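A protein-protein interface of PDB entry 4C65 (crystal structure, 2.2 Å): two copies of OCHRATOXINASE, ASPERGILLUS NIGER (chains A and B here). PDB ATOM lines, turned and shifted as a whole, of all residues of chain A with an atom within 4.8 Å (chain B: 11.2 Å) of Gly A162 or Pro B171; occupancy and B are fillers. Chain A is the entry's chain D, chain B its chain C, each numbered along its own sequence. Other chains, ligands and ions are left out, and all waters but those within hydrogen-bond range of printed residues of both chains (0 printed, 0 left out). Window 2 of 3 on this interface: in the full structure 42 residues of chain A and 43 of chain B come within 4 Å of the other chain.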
ATOM      1  N   ALA A 157      11.254   5.484 -18.060  1.00  0.00           N
ATOM      2  CA  ALA A 157      11.373   4.069 -18.349  1.00  0.00           C
ATOM      3  C   ALA A 157      12.367   3.797 -19.494  1.00  0.00           C
ATOM      4  O   ALA A 157      13.016   2.751 -19.507  1.00  0.00           O
ATOM      5  CB  ALA A 157      10.004   3.484 -18.651  1.00  0.00           C
ATOM      6  N   GLY A 158      12.484   4.715 -20.448  1.00  0.00           N
ATOM      7  CA  GLY A 158      13.369   4.485 -21.585  1.00  0.00           C
ATOM      8  C   GLY A 158      14.817   4.408 -21.173  1.00  0.00           C
ATOM      9  O   GLY A 158      15.606   3.631 -21.726  1.00  0.00           O
ATOM     10  N   GLU A 159      15.182   5.236 -20.208  1.00  0.00           N
ATOM     11  CA  GLU A 159      16.549   5.273 -19.700  1.00  0.00           C
ATOM     12  C   GLU A 159      16.881   3.963 -19.019  1.00  0.00           C
ATOM     13  O   GLU A 159      17.965   3.425 -19.208  1.00  0.00           O
ATOM     14  CB  GLU A 159      16.742   6.441 -18.716  1.00  0.00           C
ATOM     15  CG  GLU A 159      16.870   7.834 -19.358  1.00  0.00           C
ATOM     16  CD  GLU A 159      15.567   8.382 -19.931  1.00  0.00           C
ATOM     17  OE1 GLU A 159      14.497   7.758 -19.709  1.00  0.00           O
ATOM     18  OE2 GLU A 159      15.616   9.430 -20.615  1.00  0.00           O
ATOM     19  N   VAL A 160      15.947   3.457 -18.222  1.00  0.00           N
ATOM     20  CA  VAL A 160      16.196   2.240 -17.456  1.00  0.00           C
ATOM     21  C   VAL A 160      16.269   1.037 -18.384  1.00  0.00           C
ATOM     22  O   VAL A 160      17.171   0.244 -18.287  1.00  0.00           O
ATOM     23  CB  VAL A 160      15.153   2.039 -16.343  1.00  0.00           C
ATOM     24  CG1 VAL A 160      15.409   0.745 -15.596  1.00  0.00           C
ATOM     25  CG2 VAL A 160      15.188   3.209 -15.366  1.00  0.00           C
ATOM     26  N   LEU A 161      15.320   0.904 -19.290  1.00  0.00           N
ATOM     27  CA  LEU A 161      15.325  -0.228 -20.188  1.00  0.00           C
ATOM     28  C   LEU A 161      16.384  -0.115 -21.294  1.00  0.00           C
ATOM     29  O   LEU A 161      16.841  -1.135 -21.801  1.00  0.00           O
ATOM     30  CB  LEU A 161      13.941  -0.459 -20.785  1.00  0.00           C
ATOM     31  CG  LEU A 161      13.102  -1.417 -19.965  1.00  0.00           C
ATOM     32  CD1 LEU A 161      12.372  -0.696 -18.832  1.00  0.00           C
ATOM     33  CD2 LEU A 161      12.107  -2.090 -20.879  1.00  0.00           C
ATOM     34  N   GLY A 162      16.774   1.105 -21.652  1.00  0.00           N
ATOM     35  CA  GLY A 162      17.926   1.310 -22.531  1.00  0.00           C
ATOM     36  C   GLY A 162      19.209   0.795 -21.885  1.00  0.00           C
ATOM     37  O   GLY A 162      20.031   0.172 -22.543  1.00  0.00           O
ATOM     38  N   SER A 163      19.356   1.051 -20.586  1.00  0.00           N
ATOM     39  CA  SER A 163      20.497   0.548 -19.818  1.00  0.00           C
ATOM     40  C   SER A 163      20.441  -0.972 -19.543  1.00  0.00           C
ATOM     41  O   SER A 163      21.427  -1.654 -19.736  1.00  0.00           O
ATOM     42  CB  SER A 163      20.622   1.298 -18.478  1.00  0.00           C
ATOM     43  OG  SER A 163      21.063   2.635 -18.680  1.00  0.00           O
ATOM     44  N   TYR A 164      19.298  -1.487 -19.109  1.00  0.00           N
ATOM     45  CA  TYR A 164      19.244  -2.818 -18.537  1.00  0.00           C
ATOM     46  C   TYR A 164      18.352  -3.820 -19.239  1.00  0.00           C
ATOM     47  O   TYR A 164      18.294  -4.968 -18.819  1.00  0.00           O
ATOM     48  CB  TYR A 164      18.799  -2.707 -17.083  1.00  0.00           C
ATOM     49  CG  TYR A 164      19.726  -1.871 -16.245  1.00  0.00           C
ATOM     50  CD1 TYR A 164      21.116  -1.999 -16.350  1.00  0.00           C
ATOM     51  CD2 TYR A 164      19.225  -0.992 -15.314  1.00  0.00           C
ATOM     52  CE1 TYR A 164      21.964  -1.243 -15.566  1.00  0.00           C
ATOM     53  CE2 TYR A 164      20.073  -0.236 -14.525  1.00  0.00           C
ATOM     54  CZ  TYR A 164      21.445  -0.364 -14.660  1.00  0.00           C
ATOM     55  OH  TYR A 164      22.279   0.383 -13.860  1.00  0.00           O
ATOM     56  N   GLY A 165      17.649  -3.395 -20.287  1.00  0.00           N
ATOM     57  CA  GLY A 165      16.770  -4.277 -21.031  1.00  0.00           C
ATOM     58  C   GLY A 165      17.571  -5.262 -21.857  1.00  0.00           C
ATOM     59  O   GLY A 165      18.785  -5.112 -22.017  1.00  0.00           O
ATOM     60  N   ARG A 170      23.931  -3.128 -28.322  1.00  0.00           N
ATOM     61  CA  ARG A 170      24.605  -1.886 -28.627  1.00  0.00           C
ATOM     62  C   ARG A 170      25.971  -1.917 -27.977  1.00  0.00           C
ATOM     63  O   ARG A 170      26.209  -2.732 -27.099  1.00  0.00           O
ATOM     64  CB  ARG A 170      23.822  -0.708 -28.027  1.00  0.00           C
ATOM     65  CG  ARG A 170      23.440  -0.938 -26.573  1.00  0.00           C
ATOM     66  CD  ARG A 170      23.182   0.345 -25.786  1.00  0.00           C
ATOM     67  NE  ARG A 170      22.723  -0.022 -24.454  1.00  0.00           N
ATOM     68  CZ  ARG A 170      23.501  -0.309 -23.414  1.00  0.00           C
ATOM     69  NH1 ARG A 170      24.824  -0.261 -23.507  1.00  0.00           N
ATOM     70  NH2 ARG A 170      22.933  -0.635 -22.249  1.00  0.00           N
ATOM     71  N   PRO A 171      26.856  -0.999 -28.371  1.00  0.00           N
ATOM     72  CA  PRO A 171      28.087  -0.830 -27.601  1.00  0.00           C
ATOM     73  C   PRO A 171      27.795  -0.396 -26.160  1.00  0.00           C
ATOM     74  O   PRO A 171      26.683   0.019 -25.867  1.00  0.00           O
ATOM     75  CB  PRO A 171      28.826   0.297 -28.334  1.00  0.00           C
ATOM     76  CG  PRO A 171      28.239   0.326 -29.715  1.00  0.00           C
ATOM     77  CD  PRO A 171      26.821  -0.168 -29.582  1.00  0.00           C
ATOM     78  N   LEU B 161      33.940   2.807 -33.457  1.00  0.00           N
ATOM     79  CA  LEU B 161      33.300   4.097 -33.364  1.00  0.00           C
ATOM     80  C   LEU B 161      31.962   4.064 -32.620  1.00  0.00           C
ATOM     81  O   LEU B 161      31.555   5.087 -32.052  1.00  0.00           O
ATOM     82  CB  LEU B 161      33.123   4.734 -34.736  1.00  0.00           C
ATOM     83  CG  LEU B 161      34.314   5.615 -35.126  1.00  0.00           C
ATOM     84  CD1 LEU B 161      35.447   4.789 -35.757  1.00  0.00           C
ATOM     85  CD2 LEU B 161      33.840   6.658 -36.095  1.00  0.00           C
ATOM     86  N   GLY B 162      31.288   2.909 -32.600  1.00  0.00           N
ATOM     87  CA  GLY B 162      30.119   2.741 -31.753  1.00  0.00           C
ATOM     88  C   GLY B 162      30.498   2.848 -30.286  1.00  0.00           C
ATOM     89  O   GLY B 162      29.777   3.437 -29.503  1.00  0.00           O
ATOM     90  N   SER B 163      31.634   2.244 -29.936  1.00  0.00           N
ATOM     91  CA  SER B 163      32.165   2.305 -28.579  1.00  0.00           C
ATOM     92  C   SER B 163      32.741   3.669 -28.197  1.00  0.00           C
ATOM     93  O   SER B 163      32.418   4.196 -27.146  1.00  0.00           O
ATOM     94  CB  SER B 163      33.230   1.239 -28.371  1.00  0.00           C
ATOM     95  OG  SER B 163      32.668  -0.077 -28.301  1.00  0.00           O
ATOM     96  N   TYR B 164      33.535   4.273 -29.068  1.00  0.00           N
ATOM     97  CA  TYR B 164      34.325   5.404 -28.673  1.00  0.00           C
ATOM     98  C   TYR B 164      34.078   6.721 -29.422  1.00  0.00           C
ATOM     99  O   TYR B 164      34.725   7.719 -29.113  1.00  0.00           O
ATOM    100  CB  TYR B 164      35.791   5.044 -28.799  1.00  0.00           C
ATOM    101  CG  TYR B 164      36.186   3.870 -27.954  1.00  0.00           C
ATOM    102  CD1 TYR B 164      35.790   3.774 -26.638  1.00  0.00           C
ATOM    103  CD2 TYR B 164      37.014   2.879 -28.456  1.00  0.00           C
ATOM    104  CE1 TYR B 164      36.200   2.724 -25.856  1.00  0.00           C
ATOM    105  CE2 TYR B 164      37.448   1.829 -27.672  1.00  0.00           C
ATOM    106  CZ  TYR B 164      37.022   1.747 -26.380  1.00  0.00           C
ATOM    107  OH  TYR B 164      37.378   0.659 -25.595  1.00  0.00           O
ATOM    108  N   GLY B 165      33.180   6.715 -30.395  1.00  0.00           N
ATOM    109  CA  GLY B 165      32.880   7.905 -31.178  1.00  0.00           C
ATOM    110  C   GLY B 165      32.083   8.896 -30.348  1.00  0.00           C
ATOM    111  O   GLY B 165      31.608   8.559 -29.269  1.00  0.00           O
ATOM    112  N   MET B 167      29.519  10.700 -31.756  1.00  0.00           N
ATOM    113  CA  MET B 167      28.158  10.734 -32.275  1.00  0.00           C
ATOM    114  C   MET B 167      27.334   9.621 -31.576  1.00  0.00           C
ATOM    115  O   MET B 167      27.886   8.767 -30.870  1.00  0.00           O
ATOM    116  CB  MET B 167      28.175  10.474 -33.791  1.00  0.00           C
ATOM    117  CG  MET B 167      28.469   8.979 -34.161  1.00  0.00           C
ATOM    118  SD  MET B 167      30.188   8.416 -33.887  1.00  0.00           S
ATOM    119  CE  MET B 167      31.003   9.288 -35.227  1.00  0.00           C
ATOM    120  N   ASN B 168      26.028   9.619 -31.821  1.00  0.00           N
ATOM    121  CA  ASN B 168      25.114   8.567 -31.338  1.00  0.00           C
ATOM    122  C   ASN B 168      25.131   8.312 -29.845  1.00  0.00           C
ATOM    123  O   ASN B 168      25.486   7.234 -29.400  1.00  0.00           O
ATOM    124  CB  ASN B 168      25.392   7.244 -32.036  1.00  0.00           C
ATOM    125  CG  ASN B 168      25.054   7.250 -33.488  1.00  0.00           C
ATOM    126  OD1 ASN B 168      24.389   8.131 -34.005  1.00  0.00           O
ATOM    127  ND2 ASN B 168      25.447   6.176 -34.138  1.00  0.00           N
ATOM    128  N   PRO B 169      24.748   9.317 -29.059  1.00  0.00           N
ATOM    129  CA  PRO B 169      24.628   9.089 -27.649  1.00  0.00           C
ATOM    130  C   PRO B 169      23.658   7.942 -27.368  1.00  0.00           C
ATOM    131  O   PRO B 169      22.676   7.760 -28.080  1.00  0.00           O
ATOM    132  CB  PRO B 169      24.118  10.439 -27.116  1.00  0.00           C
ATOM    133  CG  PRO B 169      23.542  11.145 -28.297  1.00  0.00           C
ATOM    134  CD  PRO B 169      24.418  10.706 -29.420  1.00  0.00           C
ATOM    135  N   ARG B 170      23.933   7.194 -26.314  1.00  0.00           N
ATOM    136  CA  ARG B 170      23.213   5.976 -26.025  1.00  0.00           C
ATOM    137  C   ARG B 170      23.463   5.602 -24.589  1.00  0.00           C
ATOM    138  O   ARG B 170      24.378   6.134 -23.968  1.00  0.00           O
ATOM    139  CB  ARG B 170      23.771   4.869 -26.902  1.00  0.00           C
ATOM    140  CG  ARG B 170      25.309   4.811 -26.893  1.00  0.00           C
ATOM    141  CD  ARG B 170      25.876   3.434 -27.287  1.00  0.00           C
ATOM    142  NE  ARG B 170      27.321   3.502 -27.361  1.00  0.00           N
ATOM    143  CZ  ARG B 170      28.142   3.419 -26.321  1.00  0.00           C
ATOM    144  NH1 ARG B 170      27.690   3.184 -25.097  1.00  0.00           N
ATOM    145  NH2 ARG B 170      29.448   3.563 -26.512  1.00  0.00           N
ATOM    146  N   PRO B 171      22.700   4.632 -24.061  1.00  0.00           N
ATOM    147  CA  PRO B 171      23.045   4.093 -22.766  1.00  0.00           C
ATOM    148  C   PRO B 171      24.402   3.423 -22.819  1.00  0.00           C
ATOM    149  O   PRO B 171      24.900   3.137 -23.909  1.00  0.00           O
ATOM    150  CB  PRO B 171      21.946   3.048 -22.512  1.00  0.00           C
ATOM    151  CG  PRO B 171      20.801   3.450 -23.364  1.00  0.00           C
ATOM    152  CD  PRO B 171      21.399   4.138 -24.548  1.00  0.00           C
ATOM    153  N   GLY B 172      24.971   3.145 -21.650  1.00  0.00           N
ATOM    154  CA  GLY B 172      26.176   2.334 -21.536  1.00  0.00           C
ATOM    155  C   GLY B 172      27.448   3.150 -21.367  1.00  0.00           C
ATOM    156  O   GLY B 172      28.476   2.879 -22.006  1.00  0.00           O
ATOM    157  N   TYR B 173      27.390   4.148 -20.523  1.00  0.00           N
ATOM    158  CA  TYR B 173      28.586   4.925 -20.194  1.00  0.00           C
ATOM    159  C   TYR B 173      29.261   5.487 -21.455  1.00  0.00           C
ATOM    160  O   TYR B 173      30.469   5.459 -21.597  1.00  0.00           O
ATOM    161  CB  TYR B 173      29.524   4.097 -19.299  1.00  0.00           C
ATOM    162  CG  TYR B 173      28.764   3.549 -18.104  1.00  0.00           C
ATOM    163  CD1 TYR B 173      28.346   4.405 -17.070  1.00  0.00           C
ATOM    164  CD2 TYR B 173      28.413   2.229 -18.024  1.00  0.00           C
ATOM    165  CE1 TYR B 173      27.627   3.928 -15.975  1.00  0.00           C
ATOM    166  CE2 TYR B 173      27.668   1.739 -16.937  1.00  0.00           C
ATOM    167  CZ  TYR B 173      27.267   2.607 -15.927  1.00  0.00           C
ATOM    168  OH  TYR B 173      26.537   2.142 -14.862  1.00  0.00           O
ATOM    169  N   TRP B 174      28.429   5.985 -22.372  1.00  0.00           N
ATOM    170  CA  TRP B 174      28.887   6.600 -23.611  1.00  0.00           C
ATOM    171  C   TRP B 174      29.800   7.757 -23.249  1.00  0.00           C
ATOM    172  O   TRP B 174      29.503   8.519 -22.314  1.00  0.00           O
ATOM    173  CB  TRP B 174      27.664   7.082 -24.414  1.00  0.00           C
ATOM    174  CG  TRP B 174      27.917   7.760 -25.726  1.00  0.00           C
ATOM    175  CD1 TRP B 174      28.148   7.167 -26.929  1.00  0.00           C
ATOM    176  CD2 TRP B 174      27.920   9.154 -25.959  1.00  0.00           C
ATOM    177  NE1 TRP B 174      28.314   8.117 -27.899  1.00  0.00           N
ATOM    178  CE2 TRP B 174      28.184   9.349 -27.326  1.00  0.00           C
ATOM    179  CE3 TRP B 174      27.748  10.269 -25.142  1.00  0.00           C
ATOM    180  CZ2 TRP B 174      28.252  10.615 -27.901  1.00  0.00           C
ATOM    181  CZ3 TRP B 174      27.807  11.531 -25.723  1.00  0.00           C
ATOM    182  CH2 TRP B 174      28.046  11.689 -27.095  1.00  0.00           C
ATOM    183  N   GLY B 175      30.887   7.894 -23.981  1.00  0.00           N
ATOM    184  CA  GLY B 175      31.792   9.021 -23.792  1.00  0.00           C
ATOM    185  C   GLY B 175      32.763   8.839 -22.637  1.00  0.00           C
ATOM    186  O   GLY B 175      33.417   9.807 -22.247  1.00  0.00           O
ATOM    187  N   ALA B 176      32.840   7.626 -22.071  1.00  0.00           N
ATOM    188  CA  ALA B 176      33.684   7.410 -20.896  1.00  0.00           C
ATOM    189  C   ALA B 176      34.487   6.143 -20.966  1.00  0.00           C
ATOM    190  O   ALA B 176      34.375   5.263 -20.117  1.00  0.00           O
ATOM    191  CB  ALA B 176      32.856   7.466 -19.628  1.00  0.00           C
ATOM    192  N   GLY B 177      35.292   6.042 -22.011  1.00  0.00           N
ATOM    193  CA  GLY B 177      36.190   4.901 -22.191  1.00  0.00           C
ATOM    194  C   GLY B 177      37.644   5.335 -22.211  1.00  0.00           C
ATOM    195  O   GLY B 177      37.950   6.493 -21.937  1.00  0.00           O
ATOM    196  N   ARG B 197      34.199  16.664 -18.929  1.00  0.00           N
ATOM    197  CA  ARG B 197      32.973  16.195 -18.266  1.00  0.00           C
ATOM    198  C   ARG B 197      33.261  15.180 -17.152  1.00  0.00           C
ATOM    199  O   ARG B 197      32.621  15.236 -16.100  1.00  0.00           O
ATOM    200  CB  ARG B 197      31.982  15.583 -19.277  1.00  0.00           C
ATOM    201  CG  ARG B 197      30.569  15.410 -18.715  1.00  0.00           C
ATOM    202  CD  ARG B 197      29.521  14.735 -19.590  1.00  0.00           C
ATOM    203  NE  ARG B 197      28.795  13.792 -18.751  1.00  0.00           N
ATOM    204  CZ  ARG B 197      27.528  13.911 -18.443  1.00  0.00           C
ATOM    205  NH1 ARG B 197      26.822  14.918 -18.893  1.00  0.00           N
ATOM    206  NH2 ARG B 197      26.974  12.999 -17.685  1.00  0.00           N
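Printed residues of chain A that touch a printed residue of chain B: Gly A162, Ser A163, Arg A170 and Pro A171.
Hydrophobic or aromatic side chains of chain A that line the printed part of chain B: Pro A171.
Along chain A the printed residues that touch a printed residue of chain B span positions 162 to 171.
Printed residues of chain B that touch a printed residue of chain A: Gly B162, Ser B163, Arg B170, Pro B171 and Gly B172.
Hydrophobic or aromatic side chains of chain B within 4 Å of the printed part of chain A: Pro B171.
Along chain B the printed residues that touch a printed residue of chain A span positions 162 to 172.
Among the printed residues, no Asp or Glu carboxylate lies within 4 Å of a Lys or Arg side-chain nitrogen of the other chain.
The guanidinium group of Arg A170 is in hydrogen-bond range of the backbone carbonyl oxygen of Gly A162.
NH2 of Arg B170 is in hydrogen-bond range of O of Gly B162 (3.0 Å).
The backbone carbonyl oxygen of Glu A159 sits at hydrogen-bond distance from the side-chain hydroxyl of Ser A163 (3.2 Å).
NH1 of Arg B170 sits at hydrogen-bond distance from O of Gly B172, 3.2 Å away.
NH2 of Arg A170 lies within hydrogen-bond range of O of Ser A163, at 3.1 Å.
The backbone carbonyl oxygen (O) of Ser B163 is in hydrogen-bond range of the guanidinium group (NH2) of Arg B170.
Among the printed residues, merely in contact across the chains: Gly A162 with Pro B171 (3.4 Å), Ser A163 with Pro B171 (3.8 Å), Arg A170 with Gly B172 (3.5 Å), Pro A171 with Gly B162 (3.4 Å) and Pro A171 with Ser B163 (3.8 Å).
O of Pro B171 sits at hydrogen-bond distance from NH1 of Arg A170, 3.4 Å away.
NH1 of Arg B170 lies within hydrogen-bond range of O of Pro A171 (3.4 Å).
Of chain B, only Pro B171 comes within 4 Å of Gly A162.
Of chain A, only Gly A162, Ser A163 and Arg A170 come within 4 Å of Pro B171.
Gly A158 touches none of the printed residues of chain B.
Ser A163 touches just one residue of chain B: Pro B171 (3.8 Å).
Printed residues of chain B within 4 Å of Arg A170: Pro B171 and Gly B172.
Of the printed residues of chain A, Arg B170 touches Pro A171.
Of the printed residues of chain B, Pro A171 touches Gly B162 (3.4 Å), Ser B163 (3.8 Å) and Arg B170 (3.4 Å).
Of the printed residues of chain A, Ser B163 touches Pro A171.
The nearest printed residue of chain B that does not touch Arg A170 is Arg B170 (4.4 Å).
Gly A162 touches Pro B171, and with the chains exchanged Pro A171 touches Gly B162.
Ser A163 touches Pro B171, and with the chains exchanged Pro A171 touches Ser B163.
Arg A170 touches Pro B171, and with the chains exchanged Pro A171 touches Arg B170.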
